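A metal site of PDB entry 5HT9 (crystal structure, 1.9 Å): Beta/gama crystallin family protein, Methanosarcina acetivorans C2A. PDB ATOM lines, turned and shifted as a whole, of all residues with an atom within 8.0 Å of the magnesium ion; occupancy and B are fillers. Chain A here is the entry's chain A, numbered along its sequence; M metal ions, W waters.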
ATOM      1  N   LEU A  31      -7.533  11.191 -17.872  1.00  0.00           N
ATOM      2  CA  LEU A  31      -6.829   9.942 -18.102  1.00  0.00           C
ATOM      3  C   LEU A  31      -5.373  10.148 -18.515  1.00  0.00           C
ATOM      4  O   LEU A  31      -4.731   9.216 -19.011  1.00  0.00           O
ATOM      5  CB  LEU A  31      -7.566   9.110 -19.162  1.00  0.00           C
ATOM      6  CG  LEU A  31      -9.025   8.787 -18.870  1.00  0.00           C
ATOM      7  CD1 LEU A  31      -9.564   7.721 -19.832  1.00  0.00           C
ATOM      8  CD2 LEU A  31      -9.237   8.355 -17.416  1.00  0.00           C
ATOM      9  N   ASN A  32      -4.844  11.356 -18.305  1.00  0.00           N
ATOM     10  CA  ASN A  32      -3.419  11.602 -18.512  1.00  0.00           C
ATOM     11  C   ASN A  32      -2.584  10.605 -17.702  1.00  0.00           C
ATOM     12  O   ASN A  32      -2.757  10.509 -16.483  1.00  0.00           O
ATOM     13  CB  ASN A  32      -3.034  13.047 -18.147  1.00  0.00           C
ATOM     14  CG  ASN A  32      -1.534  13.343 -18.366  1.00  0.00           C
ATOM     15  OD1 ASN A  32      -0.740  12.440 -18.623  1.00  0.00           O
ATOM     16  ND2 ASN A  32      -1.163  14.604 -18.238  1.00  0.00           N
ATOM     17  N   ASP A  33      -1.700   9.887 -18.383  1.00  0.00           N
ATOM     18  CA  ASP A  33      -0.834   8.879 -17.762  1.00  0.00           C
ATOM     19  C   ASP A  33      -1.625   7.762 -17.075  1.00  0.00           C
ATOM     20  O   ASP A  33      -1.097   7.084 -16.201  1.00  0.00           O
ATOM     21  CB  ASP A  33       0.119   9.535 -16.745  1.00  0.00           C
ATOM     22  CG  ASP A  33       1.454   9.947 -17.368  1.00  0.00           C
ATOM     23  OD1 ASP A  33       1.599   9.889 -18.614  1.00  0.00           O
ATOM     24  OD2 ASP A  33       2.362  10.317 -16.586  1.00  0.00           O
ATOM     25  N   LYS A  34      -2.876   7.565 -17.472  1.00  0.00           N
ATOM     26  CA  LYS A  34      -3.702   6.500 -16.929  1.00  0.00           C
ATOM     27  C   LYS A  34      -4.285   5.585 -18.003  1.00  0.00           C
ATOM     28  O   LYS A  34      -4.993   4.636 -17.688  1.00  0.00           O
ATOM     29  CB  LYS A  34      -4.845   7.073 -16.095  1.00  0.00           C
ATOM     30  CG  LYS A  34      -4.431   7.690 -14.779  1.00  0.00           C
ATOM     31  CD  LYS A  34      -5.660   8.175 -14.035  1.00  0.00           C
ATOM     32  CE  LYS A  34      -5.296   8.704 -12.644  1.00  0.00           C
ATOM     33  NZ  LYS A  34      -6.508   9.098 -11.871  1.00  0.00           N
ATOM     34  N   TYR A  48       0.758  10.342 -27.862  1.00  0.00           N
ATOM     35  CA  TYR A  48       2.030  10.887 -27.379  1.00  0.00           C
ATOM     36  C   TYR A  48       2.232  10.661 -25.890  1.00  0.00           C
ATOM     37  O   TYR A  48       1.277  10.663 -25.116  1.00  0.00           O
ATOM     38  CB  TYR A  48       2.127  12.389 -27.623  1.00  0.00           C
ATOM     39  CG  TYR A  48       1.914  12.853 -29.037  1.00  0.00           C
ATOM     40  CD1 TYR A  48       0.629  13.015 -29.544  1.00  0.00           C
ATOM     41  CD2 TYR A  48       2.983  13.190 -29.850  1.00  0.00           C
ATOM     42  CE1 TYR A  48       0.423  13.478 -30.820  1.00  0.00           C
ATOM     43  CE2 TYR A  48       2.786  13.656 -31.143  1.00  0.00           C
ATOM     44  CZ  TYR A  48       1.499  13.795 -31.620  1.00  0.00           C
ATOM     45  OH  TYR A  48       1.269  14.266 -32.884  1.00  0.00           O
ATOM     46  N   GLU A  49       3.492  10.523 -25.471  1.00  0.00           N
ATOM     47  CA  GLU A  49       3.753  10.285 -24.055  1.00  0.00           C
ATOM     48  C   GLU A  49       3.581  11.528 -23.175  1.00  0.00           C
ATOM     49  O   GLU A  49       3.350  11.395 -21.967  1.00  0.00           O
ATOM     50  CB  GLU A  49       5.154   9.691 -23.860  1.00  0.00           C
ATOM     51  CG  GLU A  49       6.305  10.578 -24.311  1.00  0.00           C
ATOM     52  CD  GLU A  49       7.661   9.927 -24.068  1.00  0.00           C
ATOM     53  OE1 GLU A  49       7.778   9.101 -23.140  1.00  0.00           O
ATOM     54  OE2 GLU A  49       8.605  10.251 -24.810  1.00  0.00           O
ATOM     55  N   TYR A  50       3.680  12.720 -23.747  1.00  0.00           N
ATOM     56  CA  TYR A  50       3.559  13.941 -22.934  1.00  0.00           C
ATOM     57  C   TYR A  50       2.407  14.804 -23.428  1.00  0.00           C
ATOM     58  O   TYR A  50       1.956  14.658 -24.567  1.00  0.00           O
ATOM     59  CB  TYR A  50       4.854  14.758 -22.975  1.00  0.00           C
ATOM     60  CG  TYR A  50       6.082  13.990 -22.576  1.00  0.00           C
ATOM     61  CD1 TYR A  50       6.066  13.126 -21.507  1.00  0.00           C
ATOM     62  CD2 TYR A  50       7.260  14.127 -23.297  1.00  0.00           C
ATOM     63  CE1 TYR A  50       7.183  12.416 -21.144  1.00  0.00           C
ATOM     64  CE2 TYR A  50       8.387  13.420 -22.952  1.00  0.00           C
ATOM     65  CZ  TYR A  50       8.338  12.569 -21.874  1.00  0.00           C
ATOM     66  OH  TYR A  50       9.460  11.861 -21.520  1.00  0.00           O
ATOM     67  N   ILE A  51       1.919  15.707 -22.577  1.00  0.00           N
ATOM     68  CA  ILE A  51       0.813  16.567 -23.002  1.00  0.00           C
ATOM     69  C   ILE A  51       1.241  17.483 -24.127  1.00  0.00           C
ATOM     70  O   ILE A  51       2.433  17.682 -24.369  1.00  0.00           O
ATOM     71  CB  ILE A  51       0.269  17.435 -21.879  1.00  0.00           C
ATOM     72  CG1 ILE A  51       1.392  18.305 -21.309  1.00  0.00           C
ATOM     73  CG2 ILE A  51      -0.404  16.585 -20.821  1.00  0.00           C
ATOM     74  CD1 ILE A  51       0.862  19.415 -20.448  1.00  0.00           C
ATOM     75  N   GLY A  54       3.828  15.992 -27.085  1.00  0.00           N
ATOM     76  CA  GLY A  54       5.273  15.945 -26.943  1.00  0.00           C
ATOM     77  C   GLY A  54       5.838  14.555 -26.711  1.00  0.00           C
ATOM     78  O   GLY A  54       5.162  13.656 -26.204  1.00  0.00           O
ATOM     79  N   TRP A  58       3.085   6.959 -30.908  1.00  0.00           N
ATOM     80  CA  TRP A  58       2.746   5.723 -31.580  1.00  0.00           C
ATOM     81  C   TRP A  58       1.438   5.926 -32.308  1.00  0.00           C
ATOM     82  O   TRP A  58       0.535   6.546 -31.775  1.00  0.00           O
ATOM     83  CB  TRP A  58       2.646   4.581 -30.573  1.00  0.00           C
ATOM     84  CG  TRP A  58       3.886   4.424 -29.726  1.00  0.00           C
ATOM     85  CD1 TRP A  58       4.921   3.563 -29.946  1.00  0.00           C
ATOM     86  CD2 TRP A  58       4.211   5.166 -28.548  1.00  0.00           C
ATOM     87  NE1 TRP A  58       5.885   3.717 -28.966  1.00  0.00           N
ATOM     88  CE2 TRP A  58       5.464   4.696 -28.092  1.00  0.00           C
ATOM     89  CE3 TRP A  58       3.572   6.183 -27.823  1.00  0.00           C
ATOM     90  CZ2 TRP A  58       6.081   5.202 -26.961  1.00  0.00           C
ATOM     91  CZ3 TRP A  58       4.194   6.675 -26.692  1.00  0.00           C
ATOM     92  CH2 TRP A  58       5.434   6.188 -26.268  1.00  0.00           C
ATOM     93  N   PRO A  74       3.892   2.083 -23.902  1.00  0.00           N
ATOM     94  CA  PRO A  74       4.062   1.965 -22.435  1.00  0.00           C
ATOM     95  C   PRO A  74       2.767   2.220 -21.657  1.00  0.00           C
ATOM     96  O   PRO A  74       2.077   3.196 -21.946  1.00  0.00           O
ATOM     97  CB  PRO A  74       5.098   3.043 -22.125  1.00  0.00           C
ATOM     98  CG  PRO A  74       5.825   3.273 -23.396  1.00  0.00           C
ATOM     99  CD  PRO A  74       4.819   3.058 -24.497  1.00  0.00           C
ATOM    100  N   ASP A  75       2.449   1.365 -20.704  1.00  0.00           N
ATOM    101  CA  ASP A  75       1.232   1.516 -19.914  1.00  0.00           C
ATOM    102  C   ASP A  75       1.272   2.847 -19.162  1.00  0.00           C
ATOM    103  O   ASP A  75       2.351   3.336 -18.830  1.00  0.00           O
ATOM    104  CB  ASP A  75       1.074   0.359 -18.915  1.00  0.00           C
ATOM    105  CG  ASP A  75      -0.330   0.273 -18.334  1.00  0.00           C
ATOM    106  OD1 ASP A  75      -1.276   0.828 -18.939  1.00  0.00           O
ATOM    107  OD2 ASP A  75      -0.494  -0.366 -17.282  1.00  0.00           O
ATOM    108  N   ASN A  76       0.106   3.439 -18.936  1.00  0.00           N
ATOM    109  CA  ASN A  76       0.018   4.662 -18.140  1.00  0.00           C
ATOM    110  C   ASN A  76       1.000   5.745 -18.569  1.00  0.00           C
ATOM    111  O   ASN A  76       1.664   6.355 -17.726  1.00  0.00           O
ATOM    112  CB  ASN A  76       0.225   4.298 -16.670  1.00  0.00           C
ATOM    113  CG  ASN A  76      -0.837   3.353 -16.159  1.00  0.00           C
ATOM    114  OD1 ASN A  76      -1.989   3.424 -16.579  1.00  0.00           O
ATOM    115  ND2 ASN A  76      -0.456   2.445 -15.270  1.00  0.00           N
ATOM    116  N   SER A  77       1.094   5.974 -19.875  1.00  0.00           N
ATOM    117  CA  SER A  77       2.027   6.944 -20.435  1.00  0.00           C
ATOM    118  C   SER A  77       1.381   7.958 -21.373  1.00  0.00           C
ATOM    119  O   SER A  77       1.796   9.110 -21.443  1.00  0.00           O
ATOM    120  CB  SER A  77       3.143   6.223 -21.192  1.00  0.00           C
ATOM    121  OG  SER A  77       3.997   5.544 -20.279  1.00  0.00           O
ATOM    122  N   ILE A  78       0.381   7.519 -22.133  1.00  0.00           N
ATOM    123  CA  ILE A  78      -0.264   8.408 -23.090  1.00  0.00           C
ATOM    124  C   ILE A  78      -0.847   9.632 -22.385  1.00  0.00           C
ATOM    125  O   ILE A  78      -1.592   9.511 -21.422  1.00  0.00           O
ATOM    126  CB  ILE A  78      -1.359   7.681 -23.873  1.00  0.00           C
ATOM    127  CG1 ILE A  78      -0.738   6.535 -24.671  1.00  0.00           C
ATOM    128  CG2 ILE A  78      -2.068   8.670 -24.790  1.00  0.00           C
ATOM    129  CD1 ILE A  78      -1.738   5.656 -25.373  1.00  0.00           C
ATOM    130  N   SER A  79      -0.466  10.811 -22.863  1.00  0.00           N
ATOM    131  CA  SER A  79      -0.821  12.059 -22.209  1.00  0.00           C
ATOM    132  C   SER A  79      -1.496  13.036 -23.168  1.00  0.00           C
ATOM    133  O   SER A  79      -2.043  14.054 -22.736  1.00  0.00           O
ATOM    134  CB  SER A  79       0.428  12.713 -21.586  1.00  0.00           C
ATOM    135  OG  SER A  79       0.954  11.908 -20.540  1.00  0.00           O
ATOM    136  N   SER A  80      -1.431  12.753 -24.465  1.00  0.00           N
ATOM    137  CA  SER A  80      -2.228  13.478 -25.444  1.00  0.00           C
ATOM    138  C   SER A  80      -2.399  12.610 -26.677  1.00  0.00           C
ATOM    139  O   SER A  80      -1.646  11.658 -26.882  1.00  0.00           O
ATOM    140  CB  SER A  80      -1.587  14.827 -25.811  1.00  0.00           C
ATOM    141  OG  SER A  80      -0.246  14.651 -26.226  1.00  0.00           O
HETATM  142 MG    MG M   1       2.614  10.657 -20.281  1.00  0.00          MG
HETATM  143  O   HOH W   1       4.296   9.544 -19.977  1.00  0.00           O
HETATM  144  O   HOH W   2       3.471  12.282 -19.154  1.00  0.00           O
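Within 4 Å of the magnesium ion: Asp 33, Glu 49, Ser 77 and Ser 79.
The backbone carbonyl oxygen (O) of Glu 49 binds the magnesium ion (2.0 Å). Water W1 is bound to the magnesium ion, at 2.0 Å. The side-chain hydroxyl (OG) of Ser 79 binds the magnesium ion (2.1 Å). The magnesium ion is bound by OD1 of Asp 33, 2.1 Å away. The backbone carbonyl oxygen (O) of Ser 77 is bound to the magnesium ion, 2.1 Å away. Water W2 is bound to the magnesium ion, 2.2 Å away.
OG of Ser 79 lies close to OD1 of Asn 32, at 2.6 Å. The backbone NH (N) of Ser 79 lies within hydrogen-bond range of the backbone carbonyl oxygen (O) of Tyr 48, 2.9 Å away. The side-chain carboxylate of Asp 33 sits close to the side-chain amide oxygen of Asn 32 (3.5 Å). N of Asp 33 lies within hydrogen-bond range of O of Ile 78 (3.1 Å). OG of Ser 77 lies within hydrogen-bond range of O of Asp 75. OG of Ser 77 sits close to O of Pro 74 (3.5 Å).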
